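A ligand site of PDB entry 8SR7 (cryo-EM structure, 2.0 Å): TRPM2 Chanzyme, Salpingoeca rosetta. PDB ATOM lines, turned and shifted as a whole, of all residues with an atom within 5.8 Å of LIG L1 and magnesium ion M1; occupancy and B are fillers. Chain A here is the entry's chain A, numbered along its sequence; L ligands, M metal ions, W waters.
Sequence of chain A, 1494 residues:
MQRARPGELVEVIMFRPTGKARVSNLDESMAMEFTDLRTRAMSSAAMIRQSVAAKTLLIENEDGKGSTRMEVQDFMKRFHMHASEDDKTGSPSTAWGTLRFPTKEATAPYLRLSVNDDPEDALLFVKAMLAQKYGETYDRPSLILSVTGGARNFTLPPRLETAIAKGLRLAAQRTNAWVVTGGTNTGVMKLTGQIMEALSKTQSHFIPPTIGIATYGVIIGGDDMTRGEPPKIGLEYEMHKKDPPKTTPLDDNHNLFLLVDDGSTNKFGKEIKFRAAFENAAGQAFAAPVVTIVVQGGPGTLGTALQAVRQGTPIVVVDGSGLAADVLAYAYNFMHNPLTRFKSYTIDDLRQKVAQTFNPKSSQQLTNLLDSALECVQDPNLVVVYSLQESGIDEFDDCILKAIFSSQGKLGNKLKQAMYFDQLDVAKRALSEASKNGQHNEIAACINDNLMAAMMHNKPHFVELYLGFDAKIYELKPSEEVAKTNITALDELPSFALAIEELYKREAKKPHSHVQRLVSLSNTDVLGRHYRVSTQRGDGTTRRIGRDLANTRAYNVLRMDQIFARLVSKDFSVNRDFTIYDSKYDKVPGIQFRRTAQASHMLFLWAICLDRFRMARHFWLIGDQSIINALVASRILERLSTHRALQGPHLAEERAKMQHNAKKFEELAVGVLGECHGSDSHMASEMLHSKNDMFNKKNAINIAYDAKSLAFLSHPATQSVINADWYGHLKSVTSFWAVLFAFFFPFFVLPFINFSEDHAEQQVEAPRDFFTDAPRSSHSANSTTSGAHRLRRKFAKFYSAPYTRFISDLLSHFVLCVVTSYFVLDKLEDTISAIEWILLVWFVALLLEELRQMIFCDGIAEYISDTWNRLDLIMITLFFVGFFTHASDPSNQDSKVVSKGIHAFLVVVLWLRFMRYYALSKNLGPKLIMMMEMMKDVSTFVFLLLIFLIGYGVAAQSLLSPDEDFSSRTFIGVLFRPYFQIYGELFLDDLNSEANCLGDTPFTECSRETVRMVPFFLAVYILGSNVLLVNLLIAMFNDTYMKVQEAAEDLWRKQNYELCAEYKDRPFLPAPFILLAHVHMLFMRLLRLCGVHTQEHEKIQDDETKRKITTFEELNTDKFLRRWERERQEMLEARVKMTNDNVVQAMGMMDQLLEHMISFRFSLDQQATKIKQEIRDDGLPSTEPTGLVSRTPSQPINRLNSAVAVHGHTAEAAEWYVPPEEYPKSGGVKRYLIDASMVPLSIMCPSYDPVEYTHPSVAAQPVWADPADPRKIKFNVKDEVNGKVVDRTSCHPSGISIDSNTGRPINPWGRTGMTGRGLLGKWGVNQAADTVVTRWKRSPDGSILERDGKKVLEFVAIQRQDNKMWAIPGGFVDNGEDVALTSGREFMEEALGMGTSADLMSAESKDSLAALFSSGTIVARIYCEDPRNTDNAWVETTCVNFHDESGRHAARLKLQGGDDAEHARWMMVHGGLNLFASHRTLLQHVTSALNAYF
The side-chain carboxylate (OD2) of Asp 1460 sits close to an oxygen (O5) of LIG L1, 2.8 Å away.
Merely in contact with LIG L1: Phe 1372, Val 1435, Asp 1426, Gly 1371 and Phe 1476.
Of the 23 residues printed, 12 come within 4 Å of LIG L1.
Water W1 lies within hydrogen-bond range of the side-chain carboxylate of Glu 1386 (2.7 Å) and the side-chain carboxylate of Asp 1460 (3.1 Å).
O6 of LIG L1 sits close to O1 of LG2 L2, 2.8 Å away.
OD2 of Asp 1460 touches magnesium ion M1, 3.0 Å away.
Of the 23 residues printed, 3 come within 4 Å of magnesium ion M1.
The nearest printed residue that does not touch magnesium ion M1 is Gly 1371 (4.3 Å).
Magnesium ion M1 is bound by the side-chain carboxylate (OE1) of Glu 1390 (2.1 Å), an oxygen (O5) of LIG L1 (2.1 Å), the backbone carbonyl oxygen (O) of Gly 1370 (2.3 Å) and the side-chain carboxylate (OE2) of Glu 1390 (2.3 Å).
Magnesium ion M1 has four donor atoms within binding distance.
Slightly farther from magnesium ion M1 lies water W1 (2.7 Å).
The side-chain carboxylate (OD1) of Asp 1330 sits at hydrogen-bond distance from the side-chain hydroxyl (OG1) of Thr 1437.
A ring nitrogen (ND1) of His 1479 lies close to the backbone carbonyl oxygen (O) of Phe 1476 (3.3 Å).
The backbone NH (N) of Ile 1368 sits at hydrogen-bond distance from a ring nitrogen (ND1) of His 1479 (3.1 Å).
NH2 of Arg 1428 lies within salt-bridge range of OD2 of Asp 1426 (2.6 Å).
The guanidinium group (NH2) of Arg 1360 is in salt-bridge range of the side-chain carboxylate (OD2) of Asp 1362 (3.0 Å).
O of Val 1435 is in hydrogen-bond range of N of Cys 1424.
N of Thr 1437 sits close to SG of Cys 1424 (3.5 Å).
The backbone carbonyl oxygen (O) of Gly 1371 sits at hydrogen-bond distance from the backbone NH (N) of Ala 1329, 2.9 Å away.
OD2 of Asp 1330 is in hydrogen-bond range of O3 of LIG L1 (2.4 Å).
A ring nitrogen (NE2) of His 1479 is in hydrogen-bond range of an oxygen (O2) of LIG L1, 2.5 Å away.
The guanidinium group (NH1) of Arg 1428 is in salt-bridge range of an oxygen (O6) of LIG L1, 3.2 Å away.
NH2 of Arg 1360 lies within salt-bridge range of O6 of LIG L1 (3.0 Å).
The side-chain sulfur (SG) of Cys 1424 sits close to an oxygen (O8) of LIG L1.
NH2 of Arg 1360 lies within salt-bridge range of O1 of LG2 L2 (3.5 Å).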
ATOM      1  N   ALA A1328      10.334 -24.979   1.930  1.00  0.00           N
ATOM      2  CA  ALA A1328      10.426 -23.767   2.717  1.00  0.00           C
ATOM      3  C   ALA A1328      11.889 -23.453   2.943  1.00  0.00           C
ATOM      4  O   ALA A1328      12.730 -24.354   3.002  1.00  0.00           O
ATOM      5  CB  ALA A1328       9.697 -23.904   4.058  1.00  0.00           C
ATOM      6  N   ALA A1329      12.190 -22.173   3.044  1.00  0.00           N
ATOM      7  CA  ALA A1329      13.531 -21.712   3.369  1.00  0.00           C
ATOM      8  C   ALA A1329      13.439 -20.909   4.656  1.00  0.00           C
ATOM      9  O   ALA A1329      12.594 -20.019   4.774  1.00  0.00           O
ATOM     10  CB  ALA A1329      14.113 -20.873   2.246  1.00  0.00           C
ATOM     11  N   ASP A1330      14.289 -21.253   5.608  1.00  0.00           N
ATOM     12  CA  ASP A1330      14.400 -20.537   6.873  1.00  0.00           C
ATOM     13  C   ASP A1330      15.744 -19.837   6.981  1.00  0.00           C
ATOM     14  O   ASP A1330      16.772 -20.379   6.562  1.00  0.00           O
ATOM     15  CB  ASP A1330      14.166 -21.467   8.057  1.00  0.00           C
ATOM     16  CG  ASP A1330      12.760 -22.012   8.081  1.00  0.00           C
ATOM     17  OD1 ASP A1330      12.517 -23.039   7.441  1.00  0.00           O
ATOM     18  OD2 ASP A1330      11.893 -21.408   8.740  1.00  0.00           O
ATOM     19  N   ILE A1358      10.831 -13.978  15.082  1.00  0.00           N
ATOM     20  CA  ILE A1358       9.615 -13.243  14.780  1.00  0.00           C
ATOM     21  C   ILE A1358       8.411 -13.903  15.449  1.00  0.00           C
ATOM     22  O   ILE A1358       8.412 -15.099  15.768  1.00  0.00           O
ATOM     23  CB  ILE A1358       9.410 -13.104  13.249  1.00  0.00           C
ATOM     24  CG1 ILE A1358       9.220 -14.471  12.588  1.00  0.00           C
ATOM     25  CG2 ILE A1358      10.517 -12.284  12.639  1.00  0.00           C
ATOM     26  CD1 ILE A1358       8.433 -14.449  11.374  1.00  0.00           C
ATOM     27  N   ARG A1360       4.751 -14.902  14.938  1.00  0.00           N
ATOM     28  CA  ARG A1360       3.860 -15.191  13.819  1.00  0.00           C
ATOM     29  C   ARG A1360       2.474 -14.588  13.986  1.00  0.00           C
ATOM     30  O   ARG A1360       1.963 -14.461  15.105  1.00  0.00           O
ATOM     31  CB  ARG A1360       3.743 -16.696  13.608  1.00  0.00           C
ATOM     32  CG  ARG A1360       5.058 -17.367  13.343  1.00  0.00           C
ATOM     33  CD  ARG A1360       4.844 -18.840  13.132  1.00  0.00           C
ATOM     34  NE  ARG A1360       3.826 -19.110  12.125  1.00  0.00           N
ATOM     35  CZ  ARG A1360       4.051 -19.209  10.821  1.00  0.00           C
ATOM     36  NH1 ARG A1360       5.258 -19.036  10.317  1.00  0.00           N
ATOM     37  NH2 ARG A1360       3.042 -19.469   9.999  1.00  0.00           N
ATOM     38  N   ASP A1362      -0.379 -15.782  12.618  1.00  0.00           N
ATOM     39  CA  ASP A1362      -1.473 -16.762  12.660  1.00  0.00           C
ATOM     40  C   ASP A1362      -1.641 -17.447  14.022  1.00  0.00           C
ATOM     41  O   ASP A1362      -2.772 -17.584  14.503  1.00  0.00           O
ATOM     42  CB  ASP A1362      -1.319 -17.745  11.489  1.00  0.00           C
ATOM     43  CG  ASP A1362       0.002 -18.542  11.486  1.00  0.00           C
ATOM     44  OD1 ASP A1362       0.893 -18.333  12.334  1.00  0.00           O
ATOM     45  OD2 ASP A1362       0.140 -19.408  10.592  1.00  0.00           O
ATOM     46  N   ILE A1368      11.534 -18.818  13.594  1.00  0.00           N
ATOM     47  CA  ILE A1368      12.591 -18.371  12.678  1.00  0.00           C
ATOM     48  C   ILE A1368      11.912 -17.764  11.451  1.00  0.00           C
ATOM     49  O   ILE A1368      10.832 -18.267  11.074  1.00  0.00           O
ATOM     50  CB  ILE A1368      13.469 -19.573  12.304  1.00  0.00           C
ATOM     51  CG1 ILE A1368      14.308 -20.034  13.495  1.00  0.00           C
ATOM     52  CG2 ILE A1368      14.420 -19.309  11.165  1.00  0.00           C
ATOM     53  CD1 ILE A1368      14.919 -21.403  13.333  1.00  0.00           C
ATOM     54  N   PRO A1369      12.366 -16.581  10.960  1.00  0.00           N
ATOM     55  CA  PRO A1369      11.837 -16.018   9.700  1.00  0.00           C
ATOM     56  C   PRO A1369      12.069 -16.946   8.515  1.00  0.00           C
ATOM     57  O   PRO A1369      13.128 -17.562   8.388  1.00  0.00           O
ATOM     58  CB  PRO A1369      12.623 -14.723   9.533  1.00  0.00           C
ATOM     59  CG  PRO A1369      13.119 -14.394  10.864  1.00  0.00           C
ATOM     60  CD  PRO A1369      13.344 -15.672  11.575  1.00  0.00           C
ATOM     61  N   GLY A1370      11.094 -17.031   7.633  1.00  0.00           N
ATOM     62  CA  GLY A1370      11.218 -17.905   6.498  1.00  0.00           C
ATOM     63  C   GLY A1370       9.875 -18.066   5.829  1.00  0.00           C
ATOM     64  O   GLY A1370       8.834 -17.667   6.345  1.00  0.00           O
ATOM     65  N   GLY A1371       9.911 -18.745   4.689  1.00  0.00           N
ATOM     66  CA  GLY A1371       8.685 -18.911   3.936  1.00  0.00           C
ATOM     67  C   GLY A1371       8.880 -19.871   2.798  1.00  0.00           C
ATOM     68  O   GLY A1371       9.984 -20.397   2.597  1.00  0.00           O
ATOM     69  N   PHE A1372       7.775 -20.166   2.123  1.00  0.00           N
ATOM     70  CA  PHE A1372       7.736 -21.114   1.024  1.00  0.00           C
ATOM     71  C   PHE A1372       8.488 -20.605  -0.190  1.00  0.00           C
ATOM     72  O   PHE A1372       8.497 -19.404  -0.487  1.00  0.00           O
ATOM     73  CB  PHE A1372       6.294 -21.427   0.658  1.00  0.00           C
ATOM     74  CG  PHE A1372       5.548 -22.133   1.743  1.00  0.00           C
ATOM     75  CD1 PHE A1372       5.818 -23.479   2.017  1.00  0.00           C
ATOM     76  CD2 PHE A1372       4.603 -21.437   2.511  1.00  0.00           C
ATOM     77  CE1 PHE A1372       5.132 -24.148   3.036  1.00  0.00           C
ATOM     78  CE2 PHE A1372       3.918 -22.085   3.551  1.00  0.00           C
ATOM     79  CZ  PHE A1372       4.177 -23.450   3.803  1.00  0.00           C
ATOM     80  N   GLU A1386      12.529 -13.319   2.246  1.00  0.00           N
ATOM     81  CA  GLU A1386      11.622 -13.559   3.374  1.00  0.00           C
ATOM     82  C   GLU A1386      12.148 -12.905   4.655  1.00  0.00           C
ATOM     83  O   GLU A1386      11.332 -12.531   5.506  1.00  0.00           O
ATOM     84  CB  GLU A1386      11.315 -15.038   3.589  1.00  0.00           C
ATOM     85  CG  GLU A1386      10.418 -15.718   2.500  1.00  0.00           C
ATOM     86  CD  GLU A1386       9.109 -15.029   2.163  1.00  0.00           C
ATOM     87  OE1 GLU A1386       8.383 -14.545   3.058  1.00  0.00           O
ATOM     88  OE2 GLU A1386       8.780 -14.967   0.962  1.00  0.00           O
ATOM     89  N   GLU A1390       9.869 -10.170   6.454  1.00  0.00           N
ATOM     90  CA  GLU A1390       9.254 -10.490   7.745  1.00  0.00           C
ATOM     91  C   GLU A1390       9.977  -9.849   8.934  1.00  0.00           C
ATOM     92  O   GLU A1390       9.352  -9.154   9.746  1.00  0.00           O
ATOM     93  CB  GLU A1390       9.157 -12.013   7.911  1.00  0.00           C
ATOM     94  CG  GLU A1390       8.173 -12.600   6.916  1.00  0.00           C
ATOM     95  CD  GLU A1390       8.046 -14.089   7.009  1.00  0.00           C
ATOM     96  OE1 GLU A1390       7.696 -14.612   8.083  1.00  0.00           O
ATOM     97  OE2 GLU A1390       8.273 -14.771   6.004  1.00  0.00           O
ATOM     98  N   CYS A1424       9.483 -30.857   8.356  1.00  0.00           N
ATOM     99  CA  CYS A1424       9.037 -29.887   9.356  1.00  0.00           C
ATOM    100  C   CYS A1424       7.813 -30.390  10.124  1.00  0.00           C
ATOM    101  O   CYS A1424       6.841 -30.737   9.494  1.00  0.00           O
ATOM    102  CB  CYS A1424       8.692 -28.595   8.651  1.00  0.00           C
ATOM    103  SG  CYS A1424      10.129 -27.817   7.887  1.00  0.00           S
ATOM    104  N   ASP A1426       5.271 -29.214  11.268  1.00  0.00           N
ATOM    105  CA  ASP A1426       4.292 -28.179  10.974  1.00  0.00           C
ATOM    106  C   ASP A1426       2.894 -28.742  11.125  1.00  0.00           C
ATOM    107  O   ASP A1426       2.625 -29.833  10.603  1.00  0.00           O
ATOM    108  CB  ASP A1426       4.544 -27.680   9.537  1.00  0.00           C
ATOM    109  CG  ASP A1426       3.833 -26.368   9.188  1.00  0.00           C
ATOM    110  OD1 ASP A1426       3.107 -25.768   9.985  1.00  0.00           O
ATOM    111  OD2 ASP A1426       4.039 -25.899   8.060  1.00  0.00           O
ATOM    112  N   ARG A1428       0.097 -27.857   9.765  1.00  0.00           N
ATOM    113  CA  ARG A1428      -0.634 -27.819   8.506  1.00  0.00           C
ATOM    114  C   ARG A1428      -0.316 -28.975   7.580  1.00  0.00           C
ATOM    115  O   ARG A1428      -0.874 -29.004   6.474  1.00  0.00           O
ATOM    116  CB  ARG A1428      -0.349 -26.513   7.763  1.00  0.00           C
ATOM    117  CG  ARG A1428      -0.596 -25.255   8.561  1.00  0.00           C
ATOM    118  CD  ARG A1428       0.073 -24.072   7.894  1.00  0.00           C
ATOM    119  NE  ARG A1428       1.521 -24.118   8.036  1.00  0.00           N
ATOM    120  CZ  ARG A1428       2.347 -23.185   7.591  1.00  0.00           C
ATOM    121  NH1 ARG A1428       1.900 -22.117   6.954  1.00  0.00           N
ATOM    122  NH2 ARG A1428       3.659 -23.323   7.786  1.00  0.00           N
ATOM    123  N   VAL A1435       5.525 -29.909   4.478  1.00  0.00           N
ATOM    124  CA  VAL A1435       6.550 -28.870   4.382  1.00  0.00           C
ATOM    125  C   VAL A1435       7.910 -29.472   4.703  1.00  0.00           C
ATOM    126  O   VAL A1435       8.059 -30.172   5.720  1.00  0.00           O
ATOM    127  CB  VAL A1435       6.201 -27.704   5.328  1.00  0.00           C
ATOM    128  CG1 VAL A1435       7.163 -26.550   5.165  1.00  0.00           C
ATOM    129  CG2 VAL A1435       4.820 -27.250   5.053  1.00  0.00           C
ATOM    130  N   THR A1437      12.049 -28.174   4.934  1.00  0.00           N
ATOM    131  CA  THR A1437      12.770 -26.920   5.059  1.00  0.00           C
ATOM    132  C   THR A1437      14.246 -27.088   4.748  1.00  0.00           C
ATOM    133  O   THR A1437      14.836 -28.163   4.928  1.00  0.00           O
ATOM    134  CB  THR A1437      12.601 -26.274   6.444  1.00  0.00           C
ATOM    135  OG1 THR A1437      13.391 -25.084   6.489  1.00  0.00           O
ATOM    136  CG2 THR A1437      13.062 -27.154   7.595  1.00  0.00           C
ATOM    137  N   ASP A1460       3.717 -10.933   7.548  1.00  0.00           N
ATOM    138  CA  ASP A1460       3.062 -11.979   8.373  1.00  0.00           C
ATOM    139  C   ASP A1460       3.874 -12.189   9.644  1.00  0.00           C
ATOM    140  O   ASP A1460       4.151 -13.338   9.991  1.00  0.00           O
ATOM    141  CB  ASP A1460       2.912 -13.262   7.574  1.00  0.00           C
ATOM    142  CG  ASP A1460       4.211 -13.869   7.082  1.00  0.00           C
ATOM    143  OD1 ASP A1460       5.014 -13.130   6.505  1.00  0.00           O
ATOM    144  OD2 ASP A1460       4.411 -15.077   7.281  1.00  0.00           O
ATOM    145  N   PHE A1476       7.759 -22.469  17.121  1.00  0.00           N
ATOM    146  CA  PHE A1476       6.825 -23.041  16.151  1.00  0.00           C
ATOM    147  C   PHE A1476       7.537 -24.123  15.347  1.00  0.00           C
ATOM    148  O   PHE A1476       8.679 -23.924  14.945  1.00  0.00           O
ATOM    149  CB  PHE A1476       6.347 -21.914  15.221  1.00  0.00           C
ATOM    150  CG  PHE A1476       5.604 -22.382  14.005  1.00  0.00           C
ATOM    151  CD1 PHE A1476       4.347 -22.975  14.124  1.00  0.00           C
ATOM    152  CD2 PHE A1476       6.190 -22.223  12.731  1.00  0.00           C
ATOM    153  CE1 PHE A1476       3.652 -23.414  12.990  1.00  0.00           C
ATOM    154  CE2 PHE A1476       5.508 -22.649  11.584  1.00  0.00           C
ATOM    155  CZ  PHE A1476       4.239 -23.241  11.716  1.00  0.00           C
ATOM    156  N   ALA A1477       6.814 -25.224  15.089  1.00  0.00           N
ATOM    157  CA  ALA A1477       7.155 -26.399  14.235  1.00  0.00           C
ATOM    158  C   ALA A1477       8.447 -27.053  14.721  1.00  0.00           C
ATOM    159  O   ALA A1477       8.598 -27.245  15.942  1.00  0.00           O
ATOM    160  CB  ALA A1477       7.138 -25.990  12.757  1.00  0.00           C
ATOM    161  N   HIS A1479      11.579 -25.804  14.564  1.00  0.00           N
ATOM    162  CA  HIS A1479      12.624 -24.791  14.561  1.00  0.00           C
ATOM    163  C   HIS A1479      13.683 -24.983  15.652  1.00  0.00           C
ATOM    164  O   HIS A1479      14.786 -24.429  15.520  1.00  0.00           O
ATOM    165  CB  HIS A1479      11.999 -23.398  14.673  1.00  0.00           C
ATOM    166  CG  HIS A1479      11.302 -22.959  13.428  1.00  0.00           C
ATOM    167  ND1 HIS A1479      10.573 -21.800  13.353  1.00  0.00           N
ATOM    168  CD2 HIS A1479      11.194 -23.541  12.201  1.00  0.00           C
ATOM    169  CE1 HIS A1479      10.061 -21.668  12.146  1.00  0.00           C
ATOM    170  NE2 HIS A1479      10.426 -22.720  11.423  1.00  0.00           N
ATOM    171  N   LEU A1482      16.250 -27.048  14.017  1.00  0.00           N
ATOM    172  CA  LEU A1482      17.031 -26.151  13.149  1.00  0.00           C
ATOM    173  C   LEU A1482      18.073 -25.367  13.938  1.00  0.00           C
ATOM    174  O   LEU A1482      19.229 -25.248  13.501  1.00  0.00           O
ATOM    175  CB  LEU A1482      16.095 -25.184  12.432  1.00  0.00           C
ATOM    176  CG  LEU A1482      15.105 -25.748  11.416  1.00  0.00           C
ATOM    177  CD1 LEU A1482      14.335 -24.615  10.755  1.00  0.00           C
ATOM    178  CD2 LEU A1482      15.787 -26.602  10.407  1.00  0.00           C
HETATM  179  C1  LIG L   1       7.626 -24.120   8.738  1.00  0.00           C
HETATM  180  O1  LIG L   1       6.559 -23.288   8.073  1.00  0.00           O
HETATM  181  C2  LIG L   1       8.980 -23.535   8.108  1.00  0.00           C
HETATM  182  O2  LIG L   1      10.087 -23.617   9.132  1.00  0.00           O
HETATM  183  C3  LIG L   1       8.735 -22.368   7.771  1.00  0.00           C
HETATM  184  O3  LIG L   1       9.495 -21.389   8.576  1.00  0.00           O
HETATM  185  C4  LIG L   1       7.102 -22.117   8.007  1.00  0.00           C
HETATM  186  C5  LIG L   1       6.527 -21.338   6.874  1.00  0.00           C
HETATM  187  O4  LIG L   1       6.346 -20.016   7.288  1.00  0.00           O
HETATM  188  P1  LIG L   1       5.167 -19.142   6.558  1.00  0.00           P
HETATM  189  O5  LIG L   1       5.410 -17.672   6.785  1.00  0.00           O
HETATM  190  O6  LIG L   1       3.830 -19.535   7.114  1.00  0.00           O
HETATM  191  O7  LIG L   1       5.211 -19.437   5.076  1.00  0.00           O
HETATM  192  O8  LIG L   1       7.487 -25.344   8.437  1.00  0.00           O
HETATM  193  P1  LG2 L   2       0.951 -17.716   6.149  1.00  0.00           P
HETATM  194  O1  LG2 L   2       1.940 -17.523   7.274  1.00  0.00           O
HETATM  195  O2  LG2 L   2      -0.137 -18.703   6.503  1.00  0.00           O
HETATM  196  O3  LG2 L   2       0.393 -16.389   5.641  1.00  0.00           O
HETATM  197  O4  LG2 L   2       1.754 -18.365   4.910  1.00  0.00           O
HETATM  198  C1  LG2 L   2       2.634 -17.531   4.113  1.00  0.00           C
HETATM  199  C2  LG2 L   2       2.014 -17.290   2.751  1.00  0.00           C
HETATM  200  O5  LG2 L   2       2.849 -17.877   1.728  1.00  0.00           O
HETATM  201  C3  LG2 L   2       0.655 -17.950   2.493  1.00  0.00           C
HETATM  202  O6  LG2 L   2      -0.403 -17.164   3.027  1.00  0.00           O
HETATM  203  C4  LG2 L   2       0.605 -17.955   0.958  1.00  0.00           C
HETATM  204  O7  LG2 L   2       0.062 -16.759   0.464  1.00  0.00           O
HETATM  205  C5  LG2 L   2       2.075 -18.064   0.562  1.00  0.00           C
HETATM  206  N1  LG2 L   2       2.461 -19.319  -0.062  1.00  0.00           N
HETATM  207  C6  LG2 L   2       3.311 -19.444  -1.128  1.00  0.00           C
HETATM  208  N2  LG2 L   2       3.509 -20.683  -1.497  1.00  0.00           N
HETATM  209  C7  LG2 L   2       2.753 -21.427  -0.612  1.00  0.00           C
HETATM  210  C8  LG2 L   2       2.554 -22.809  -0.480  1.00  0.00           C
HETATM  211  N3  LG2 L   2       3.124 -23.712  -1.271  1.00  0.00           N
HETATM  212  N4  LG2 L   2       1.737 -23.235   0.504  1.00  0.00           N
HETATM  213  C9  LG2 L   2       1.168 -22.325   1.302  1.00  0.00           C
HETATM  214  N5  LG2 L   2       1.282 -20.999   1.270  1.00  0.00           N
HETATM  215  C10 LG2 L   2       2.096 -20.602   0.285  1.00  0.00           C
HETATM  216 MG    MG M   1       7.089 -16.395   7.088  1.00  0.00          MG
HETATM  217 MG    MG M   2       5.375 -17.095   3.478  1.00  0.00          MG
HETATM  218  O   HOH W   1       6.431 -15.184   4.735  1.00  0.00           O
